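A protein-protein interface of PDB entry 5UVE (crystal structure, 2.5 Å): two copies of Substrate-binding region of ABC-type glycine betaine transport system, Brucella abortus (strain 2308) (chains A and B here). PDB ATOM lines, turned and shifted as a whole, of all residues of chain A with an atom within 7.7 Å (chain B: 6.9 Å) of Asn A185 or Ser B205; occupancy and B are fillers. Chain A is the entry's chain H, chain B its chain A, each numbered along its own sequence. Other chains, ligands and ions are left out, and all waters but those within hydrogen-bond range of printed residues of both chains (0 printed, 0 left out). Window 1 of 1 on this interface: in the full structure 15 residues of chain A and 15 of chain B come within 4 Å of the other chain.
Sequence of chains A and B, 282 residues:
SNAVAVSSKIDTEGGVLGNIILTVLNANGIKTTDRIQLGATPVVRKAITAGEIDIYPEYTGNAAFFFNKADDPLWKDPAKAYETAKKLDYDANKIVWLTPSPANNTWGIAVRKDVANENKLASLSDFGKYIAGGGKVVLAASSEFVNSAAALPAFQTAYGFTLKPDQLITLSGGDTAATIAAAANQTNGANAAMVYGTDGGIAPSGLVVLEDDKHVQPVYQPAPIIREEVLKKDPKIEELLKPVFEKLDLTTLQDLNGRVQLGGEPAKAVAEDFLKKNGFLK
The backbone carbonyl oxygen of Ala B184 lies within hydrogen-bond range of the guanidinium group of Arg B112. The side-chain amide nitrogen (ND2) of Asn B185 sits at hydrogen-bond distance from the backbone carbonyl oxygen (O) of Ala B181 (2.7 Å). O of Gly B201 is in hydrogen-bond range of OG of Ser B205, 2.8 Å away. The guanidinium group (NH1) of Arg A112 lies within hydrogen-bond range of the backbone carbonyl oxygen (O) of Ala A184, 3.1 Å away. The side-chain amide nitrogen (ND2) of Asn A185 sits at hydrogen-bond distance from the backbone carbonyl oxygen (O) of Ala A181, at 2.6 Å. The backbone NH (N) of Thr A187 lies within hydrogen-bond range of the backbone carbonyl oxygen (O) of Ala A182.
Among the printed residues, merely in contact across the chains: Ala A178 with Leu B262 (3.5 Å), Ala A182 with Leu B262 (3.7 Å), Ala A184 with Asn B185 (3.99 Å), Asn A185 with Ala B184 (3.9 Å), Asn A185 with Pro B204 (3.2 Å), Asn A185 with Ser B205 (3.6 Å), Thr A187 with Pro B204 (3.6 Å), Thr A187 with Leu B262 (3.6 Å) and Ser A205 with Asn B185 (3.5 Å).
Asn A185 touches three residues of chain B. Of chain A, only Asn A185 (3.6 Å) comes within 4 Å of Ser B205. No residue of chain A comes within 4 Å of Gly B206. Printed residues of chain B within 4 Å of Ser A205: Asn B185. Printed residues of chain B within 4 Å of Ala A184: Asn B185 (3.99 Å). Printed residues of chain B within 4 Å of Thr A187: Pro B204 and Leu B262. Of the printed residues of chain B, Ala A182 touches Leu B262. Of the printed residues of chain B, Ala A178 touches Leu B262 (3.5 Å). Gln A186 touches none of the printed residues of chain B. Ile B180 touches none of the printed residues of chain A.
Hydrophobic or aromatic side chains of chain B that line the printed part of chain A: Ala B184, Pro B204 and Leu B262.
Ala A184 touches Asn B185, and with the chains exchanged Asn A185 touches Ala B184. Asn A185 touches Ser B205, and with the chains exchanged Ser A205 touches Asn B185. Positions printed for both chains: 112, 177, 180, 181, 183, 184, 185, 205 and 207. Of the 9 pairs that touch across the chains among the printed residues, 4 have their exchanged pair printed and touching as well.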
ATOM      1  N   ARG A 112     -13.977  37.462   5.971  1.00  0.00           N
ATOM      2  CA  ARG A 112     -13.607  36.704   4.784  1.00  0.00           C
ATOM      3  C   ARG A 112     -14.353  37.225   3.561  1.00  0.00           C
ATOM      4  O   ARG A 112     -15.468  37.747   3.662  1.00  0.00           O
ATOM      5  CB  ARG A 112     -13.896  35.216   5.002  1.00  0.00           C
ATOM      6  CG  ARG A 112     -13.484  34.722   6.388  1.00  0.00           C
ATOM      7  CD  ARG A 112     -13.670  33.214   6.590  1.00  0.00           C
ATOM      8  NE  ARG A 112     -13.643  32.414   5.367  1.00  0.00           N
ATOM      9  CZ  ARG A 112     -12.588  31.738   4.920  1.00  0.00           C
ATOM     10  NH1 ARG A 112     -11.441  31.756   5.585  1.00  0.00           N
ATOM     11  NH2 ARG A 112     -12.685  31.037   3.801  1.00  0.00           N
ATOM     12  N   ALA A 177      -1.876  39.034  13.991  1.00  0.00           N
ATOM     13  CA  ALA A 177      -1.579  37.937  13.077  1.00  0.00           C
ATOM     14  C   ALA A 177      -2.297  36.658  13.483  1.00  0.00           C
ATOM     15  O   ALA A 177      -2.715  35.878  12.617  1.00  0.00           O
ATOM     16  CB  ALA A 177      -0.067  37.710  13.008  1.00  0.00           C
ATOM     17  N   ALA A 178      -2.479  36.441  14.787  1.00  0.00           N
ATOM     18  CA  ALA A 178      -3.149  35.230  15.246  1.00  0.00           C
ATOM     19  C   ALA A 178      -4.642  35.276  14.941  1.00  0.00           C
ATOM     20  O   ALA A 178      -5.221  34.277  14.499  1.00  0.00           O
ATOM     21  CB  ALA A 178      -2.907  35.037  16.742  1.00  0.00           C
ATOM     22  N   THR A 179      -5.279  36.428  15.152  1.00  0.00           N
ATOM     23  CA  THR A 179      -6.690  36.551  14.801  1.00  0.00           C
ATOM     24  C   THR A 179      -6.893  36.370  13.300  1.00  0.00           C
ATOM     25  O   THR A 179      -7.835  35.695  12.873  1.00  0.00           O
ATOM     26  CB  THR A 179      -7.240  37.901  15.264  1.00  0.00           C
ATOM     27  OG1 THR A 179      -6.410  38.960  14.773  1.00  0.00           O
ATOM     28  CG2 THR A 179      -7.253  37.963  16.784  1.00  0.00           C
ATOM     29  N   ILE A 180      -5.993  36.931  12.488  1.00  0.00           N
ATOM     30  CA  ILE A 180      -6.100  36.790  11.037  1.00  0.00           C
ATOM     31  C   ILE A 180      -5.975  35.326  10.640  1.00  0.00           C
ATOM     32  O   ILE A 180      -6.707  34.833   9.774  1.00  0.00           O
ATOM     33  CB  ILE A 180      -5.025  37.643  10.335  1.00  0.00           C
ATOM     34  CG1 ILE A 180      -5.267  39.130  10.562  1.00  0.00           C
ATOM     35  CG2 ILE A 180      -5.022  37.369   8.835  1.00  0.00           C
ATOM     36  CD1 ILE A 180      -4.136  40.016  10.068  1.00  0.00           C
ATOM     37  N   ALA A 181      -5.041  34.607  11.268  1.00  0.00           N
ATOM     38  CA  ALA A 181      -4.861  33.191  10.974  1.00  0.00           C
ATOM     39  C   ALA A 181      -6.059  32.368  11.425  1.00  0.00           C
ATOM     40  O   ALA A 181      -6.355  31.327  10.827  1.00  0.00           O
ATOM     41  CB  ALA A 181      -3.578  32.677  11.632  1.00  0.00           C
ATOM     42  N   ALA A 182      -6.753  32.808  12.478  1.00  0.00           N
ATOM     43  CA  ALA A 182      -7.927  32.077  12.939  1.00  0.00           C
ATOM     44  C   ALA A 182      -9.072  32.183  11.940  1.00  0.00           C
ATOM     45  O   ALA A 182      -9.754  31.189  11.662  1.00  0.00           O
ATOM     46  CB  ALA A 182      -8.359  32.589  14.313  1.00  0.00           C
ATOM     47  N   ALA A 183      -9.303  33.374  11.389  1.00  0.00           N
ATOM     48  CA  ALA A 183     -10.373  33.529  10.410  1.00  0.00           C
ATOM     49  C   ALA A 183      -9.982  32.962   9.051  1.00  0.00           C
ATOM     50  O   ALA A 183     -10.847  32.479   8.311  1.00  0.00           O
ATOM     51  CB  ALA A 183     -10.761  35.001  10.282  1.00  0.00           C
ATOM     52  N   ALA A 184      -8.691  33.000   8.715  1.00  0.00           N
ATOM     53  CA  ALA A 184      -8.244  32.459   7.437  1.00  0.00           C
ATOM     54  C   ALA A 184      -8.398  30.941   7.401  1.00  0.00           C
ATOM     55  O   ALA A 184      -8.750  30.373   6.360  1.00  0.00           O
ATOM     56  CB  ALA A 184      -6.793  32.861   7.177  1.00  0.00           C
ATOM     57  N   ASN A 185      -8.156  30.270   8.528  1.00  0.00           N
ATOM     58  CA  ASN A 185      -8.326  28.825   8.622  1.00  0.00           C
ATOM     59  C   ASN A 185      -9.643  28.436   9.282  1.00  0.00           C
ATOM     60  O   ASN A 185      -9.921  27.242   9.419  1.00  0.00           O
ATOM     61  CB  ASN A 185      -7.157  28.202   9.397  1.00  0.00           C
ATOM     62  CG  ASN A 185      -5.800  28.640   8.867  1.00  0.00           C
ATOM     63  OD1 ASN A 185      -5.440  28.353   7.724  1.00  0.00           O
ATOM     64  ND2 ASN A 185      -5.042  29.340   9.701  1.00  0.00           N
ATOM     65  N   GLN A 186     -10.454  29.416   9.682  1.00  0.00           N
ATOM     66  CA  GLN A 186     -11.787  29.193  10.251  1.00  0.00           C
ATOM     67  C   GLN A 186     -11.717  28.329  11.507  1.00  0.00           C
ATOM     68  O   GLN A 186     -12.534  27.429  11.712  1.00  0.00           O
ATOM     69  CB  GLN A 186     -12.756  28.592   9.230  1.00  0.00           C
ATOM     70  CG  GLN A 186     -12.944  29.460   7.996  1.00  0.00           C
ATOM     71  CD  GLN A 186     -13.999  28.931   7.046  1.00  0.00           C
ATOM     72  OE1 GLN A 186     -13.734  28.716   5.866  1.00  0.00           O
ATOM     73  NE2 GLN A 186     -15.228  28.803   7.538  1.00  0.00           N
ATOM     74  N   THR A 187     -10.713  28.589  12.340  1.00  0.00           N
ATOM     75  CA  THR A 187     -10.592  27.867  13.597  1.00  0.00           C
ATOM     76  C   THR A 187     -11.774  28.210  14.497  1.00  0.00           C
ATOM     77  O   THR A 187     -12.087  29.387  14.694  1.00  0.00           O
ATOM     78  CB  THR A 187      -9.276  28.219  14.291  1.00  0.00           C
ATOM     79  OG1 THR A 187      -8.192  28.033  13.376  1.00  0.00           O
ATOM     80  CG2 THR A 187      -9.067  27.330  15.509  1.00  0.00           C
ATOM     81  N   ASN A 188     -12.429  27.178  15.032  1.00  0.00           N
ATOM     82  CA  ASN A 188     -13.649  27.328  15.826  1.00  0.00           C
ATOM     83  C   ASN A 188     -14.715  28.140  15.090  1.00  0.00           C
ATOM     84  O   ASN A 188     -15.468  28.906  15.695  1.00  0.00           O
ATOM     85  CB  ASN A 188     -13.343  27.962  17.183  1.00  0.00           C
ATOM     86  CG  ASN A 188     -12.772  26.979  18.168  1.00  0.00           C
ATOM     87  OD1 ASN A 188     -12.787  25.773  17.936  1.00  0.00           O
ATOM     88  ND2 ASN A 188     -12.275  27.487  19.289  1.00  0.00           N
ATOM     89  N   GLY A 189     -14.784  27.969  13.770  1.00  0.00           N
ATOM     90  CA  GLY A 189     -15.822  28.609  12.987  1.00  0.00           C
ATOM     91  C   GLY A 189     -15.664  30.097  12.782  1.00  0.00           C
ATOM     92  O   GLY A 189     -16.629  30.763  12.400  1.00  0.00           O
ATOM     93  N   ALA A 190     -14.477  30.646  13.023  1.00  0.00           N
ATOM     94  CA  ALA A 190     -14.289  32.086  12.908  1.00  0.00           C
ATOM     95  C   ALA A 190     -14.349  32.534  11.450  1.00  0.00           C
ATOM     96  O   ALA A 190     -13.780  31.894  10.562  1.00  0.00           O
ATOM     97  CB  ALA A 190     -12.953  32.497  13.526  1.00  0.00           C
ATOM     98  N   SER A 205      -4.626  36.241   3.061  1.00  0.00           N
ATOM     99  CA  SER A 205      -5.562  35.373   3.768  1.00  0.00           C
ATOM    100  C   SER A 205      -6.986  35.446   3.227  1.00  0.00           C
ATOM    101  O   SER A 205      -7.859  34.729   3.729  1.00  0.00           O
ATOM    102  CB  SER A 205      -5.579  35.718   5.259  1.00  0.00           C
ATOM    103  OG  SER A 205      -4.310  35.499   5.848  1.00  0.00           O
ATOM    104  N   LEU A 207      -9.121  38.240   3.240  1.00  0.00           N
ATOM    105  CA  LEU A 207      -9.942  39.017   4.157  1.00  0.00           C
ATOM    106  C   LEU A 207     -10.159  40.416   3.599  1.00  0.00           C
ATOM    107  O   LEU A 207      -9.354  40.919   2.807  1.00  0.00           O
ATOM    108  CB  LEU A 207      -9.294  39.106   5.549  1.00  0.00           C
ATOM    109  CG  LEU A 207      -9.084  37.803   6.330  1.00  0.00           C
ATOM    110  CD1 LEU A 207      -8.607  38.088   7.752  1.00  0.00           C
ATOM    111  CD2 LEU A 207     -10.353  36.963   6.346  1.00  0.00           C
ATOM    112  N   ARG B 112       1.855  20.865   3.554  1.00  0.00           N
ATOM    113  CA  ARG B 112       0.401  20.801   3.573  1.00  0.00           C
ATOM    114  C   ARG B 112      -0.034  19.341   3.494  1.00  0.00           C
ATOM    115  O   ARG B 112       0.685  18.485   2.969  1.00  0.00           O
ATOM    116  CB  ARG B 112      -0.196  21.605   2.411  1.00  0.00           C
ATOM    117  CG  ARG B 112       0.555  22.900   2.112  1.00  0.00           C
ATOM    118  CD  ARG B 112      -0.154  23.803   1.108  1.00  0.00           C
ATOM    119  NE  ARG B 112      -1.276  24.517   1.703  1.00  0.00           N
ATOM    120  CZ  ARG B 112      -2.544  24.371   1.337  1.00  0.00           C
ATOM    121  NH1 ARG B 112      -2.872  23.527   0.364  1.00  0.00           N
ATOM    122  NH2 ARG B 112      -3.487  25.072   1.949  1.00  0.00           N
ATOM    123  N   LYS B 113      -1.201  19.042   4.069  1.00  0.00           N
ATOM    124  CA  LYS B 113      -1.633  17.647   4.122  1.00  0.00           C
ATOM    125  C   LYS B 113      -1.785  17.060   2.728  1.00  0.00           C
ATOM    126  O   LYS B 113      -1.485  15.877   2.521  1.00  0.00           O
ATOM    127  CB  LYS B 113      -2.941  17.497   4.895  1.00  0.00           C
ATOM    128  CG  LYS B 113      -2.912  18.018   6.317  1.00  0.00           C
ATOM    129  CD  LYS B 113      -4.274  17.856   6.977  1.00  0.00           C
ATOM    130  CE  LYS B 113      -5.324  18.754   6.340  1.00  0.00           C
ATOM    131  NZ  LYS B 113      -6.608  18.688   7.093  1.00  0.00           N
ATOM    132  N   ALA B 177       5.258  31.483  12.757  1.00  0.00           N
ATOM    133  CA  ALA B 177       3.865  31.746  12.410  1.00  0.00           C
ATOM    134  C   ALA B 177       3.736  32.317  11.006  1.00  0.00           C
ATOM    135  O   ALA B 177       2.751  32.037  10.313  1.00  0.00           O
ATOM    136  CB  ALA B 177       3.235  32.696  13.430  1.00  0.00           C
ATOM    137  N   ILE B 180       4.322  29.460   8.454  1.00  0.00           N
ATOM    138  CA  ILE B 180       3.141  28.603   8.472  1.00  0.00           C
ATOM    139  C   ILE B 180       1.989  29.273   7.737  1.00  0.00           C
ATOM    140  O   ILE B 180       1.288  28.639   6.938  1.00  0.00           O
ATOM    141  CB  ILE B 180       2.764  28.254   9.924  1.00  0.00           C
ATOM    142  CG1 ILE B 180       3.780  27.276  10.516  1.00  0.00           C
ATOM    143  CG2 ILE B 180       1.367  27.677  10.004  1.00  0.00           C
ATOM    144  CD1 ILE B 180       3.653  27.097  12.013  1.00  0.00           C
ATOM    145  N   ALA B 181       1.803  30.577   7.966  1.00  0.00           N
ATOM    146  CA  ALA B 181       0.743  31.320   7.291  1.00  0.00           C
ATOM    147  C   ALA B 181       0.999  31.436   5.793  1.00  0.00           C
ATOM    148  O   ALA B 181       0.048  31.527   5.008  1.00  0.00           O
ATOM    149  CB  ALA B 181       0.595  32.704   7.923  1.00  0.00           C
ATOM    150  N   ALA B 183       2.478  29.074   3.873  1.00  0.00           N
ATOM    151  CA  ALA B 183       2.093  27.796   3.290  1.00  0.00           C
ATOM    152  C   ALA B 183       0.606  27.516   3.479  1.00  0.00           C
ATOM    153  O   ALA B 183      -0.003  26.828   2.653  1.00  0.00           O
ATOM    154  CB  ALA B 183       2.929  26.663   3.890  1.00  0.00           C
ATOM    155  N   ALA B 184       0.008  28.035   4.555  1.00  0.00           N
ATOM    156  CA  ALA B 184      -1.414  27.811   4.788  1.00  0.00           C
ATOM    157  C   ALA B 184      -2.264  28.509   3.733  1.00  0.00           C
ATOM    158  O   ALA B 184      -3.318  27.994   3.344  1.00  0.00           O
ATOM    159  CB  ALA B 184      -1.804  28.285   6.189  1.00  0.00           C
ATOM    160  N   ASN B 185      -1.834  29.679   3.268  1.00  0.00           N
ATOM    161  CA  ASN B 185      -2.525  30.395   2.206  1.00  0.00           C
ATOM    162  C   ASN B 185      -1.853  30.209   0.852  1.00  0.00           C
ATOM    163  O   ASN B 185      -2.338  30.748  -0.148  1.00  0.00           O
ATOM    164  CB  ASN B 185      -2.606  31.889   2.538  1.00  0.00           C
ATOM    165  CG  ASN B 185      -3.145  32.155   3.932  1.00  0.00           C
ATOM    166  OD1 ASN B 185      -4.287  31.817   4.249  1.00  0.00           O
ATOM    167  ND2 ASN B 185      -2.333  32.796   4.764  1.00  0.00           N
ATOM    168  N   GLY B 200       1.810  25.920  17.486  1.00  0.00           N
ATOM    169  CA  GLY B 200       0.367  25.998  17.634  1.00  0.00           C
ATOM    170  C   GLY B 200      -0.390  26.184  16.335  1.00  0.00           C
ATOM    171  O   GLY B 200      -1.573  25.836  16.267  1.00  0.00           O
ATOM    172  N   GLY B 201       0.258  26.716  15.306  1.00  0.00           N
ATOM    173  CA  GLY B 201      -0.421  26.937  14.049  1.00  0.00           C
ATOM    174  C   GLY B 201      -0.461  25.748  13.115  1.00  0.00           C
ATOM    175  O   GLY B 201      -1.198  25.789  12.127  1.00  0.00           O
ATOM    176  N   ILE B 202       0.306  24.693  13.401  1.00  0.00           N
ATOM    177  CA  ILE B 202       0.465  23.600  12.440  1.00  0.00           C
ATOM    178  C   ILE B 202      -0.868  22.906  12.180  1.00  0.00           C
ATOM    179  O   ILE B 202      -1.319  22.802  11.034  1.00  0.00           O
ATOM    180  CB  ILE B 202       1.534  22.604  12.927  1.00  0.00           C
ATOM    181  CG1 ILE B 202       2.897  23.297  13.027  1.00  0.00           C
ATOM    182  CG2 ILE B 202       1.586  21.386  12.011  1.00  0.00           C
ATOM    183  CD1 ILE B 202       3.996  22.420  13.598  1.00  0.00           C
ATOM    184  N   ALA B 203      -1.517  22.415  13.240  1.00  0.00           N
ATOM    185  CA  ALA B 203      -2.745  21.646  13.037  1.00  0.00           C
ATOM    186  C   ALA B 203      -3.885  22.500  12.494  1.00  0.00           C
ATOM    187  O   ALA B 203      -4.513  22.087  11.503  1.00  0.00           O
ATOM    188  CB  ALA B 203      -3.134  20.924  14.330  1.00  0.00           C
ATOM    189  N   PRO B 204      -4.203  23.674  13.052  1.00  0.00           N
ATOM    190  CA  PRO B 204      -5.297  24.473  12.468  1.00  0.00           C
ATOM    191  C   PRO B 204      -5.019  24.964  11.054  1.00  0.00           C
ATOM    192  O   PRO B 204      -5.966  25.344  10.356  1.00  0.00           O
ATOM    193  CB  PRO B 204      -5.443  25.645  13.449  1.00  0.00           C
ATOM    194  CG  PRO B 204      -4.846  25.158  14.720  1.00  0.00           C
ATOM    195  CD  PRO B 204      -3.701  24.292  14.295  1.00  0.00           C
ATOM    196  N   SER B 205      -3.763  24.978  10.610  1.00  0.00           N
ATOM    197  CA  SER B 205      -3.432  25.370   9.245  1.00  0.00           C
ATOM    198  C   SER B 205      -3.416  24.200   8.268  1.00  0.00           C
ATOM    199  O   SER B 205      -3.155  24.413   7.079  1.00  0.00           O
ATOM    200  CB  SER B 205      -2.076  26.083   9.203  1.00  0.00           C
ATOM    201  OG  SER B 205      -2.101  27.288   9.952  1.00  0.00           O
ATOM    202  N   GLY B 206      -3.660  22.975   8.731  1.00  0.00           N
ATOM    203  CA  GLY B 206      -3.659  21.829   7.842  1.00  0.00           C
ATOM    204  C   GLY B 206      -2.273  21.446   7.371  1.00  0.00           C
ATOM    205  O   GLY B 206      -2.062  21.177   6.185  1.00  0.00           O
ATOM    206  N   LEU B 207      -1.315  21.408   8.290  1.00  0.00           N
ATOM    207  CA  LEU B 207       0.062  21.080   7.963  1.00  0.00           C
ATOM    208  C   LEU B 207       0.477  19.789   8.657  1.00  0.00           C
ATOM    209  O   LEU B 207      -0.073  19.424   9.701  1.00  0.00           O
ATOM    210  CB  LEU B 207       1.002  22.216   8.383  1.00  0.00           C
ATOM    211  CG  LEU B 207       0.765  23.562   7.697  1.00  0.00           C
ATOM    212  CD1 LEU B 207       1.868  24.542   8.053  1.00  0.00           C
ATOM    213  CD2 LEU B 207       0.654  23.389   6.190  1.00  0.00           C
ATOM    214  N   LEU B 262      -4.862  29.501  18.561  1.00  0.00           N
ATOM    215  CA  LEU B 262      -5.791  29.949  17.534  1.00  0.00           C
ATOM    216  C   LEU B 262      -7.254  29.677  17.851  1.00  0.00           C
ATOM    217  O   LEU B 262      -8.123  30.333  17.264  1.00  0.00           O
ATOM    218  CB  LEU B 262      -5.459  29.290  16.187  1.00  0.00           C
ATOM    219  CG  LEU B 262      -4.088  29.629  15.596  1.00  0.00           C
ATOM    220  CD1 LEU B 262      -3.901  28.954  14.248  1.00  0.00           C
ATOM    221  CD2 LEU B 262      -3.919  31.137  15.467  1.00  0.00           C
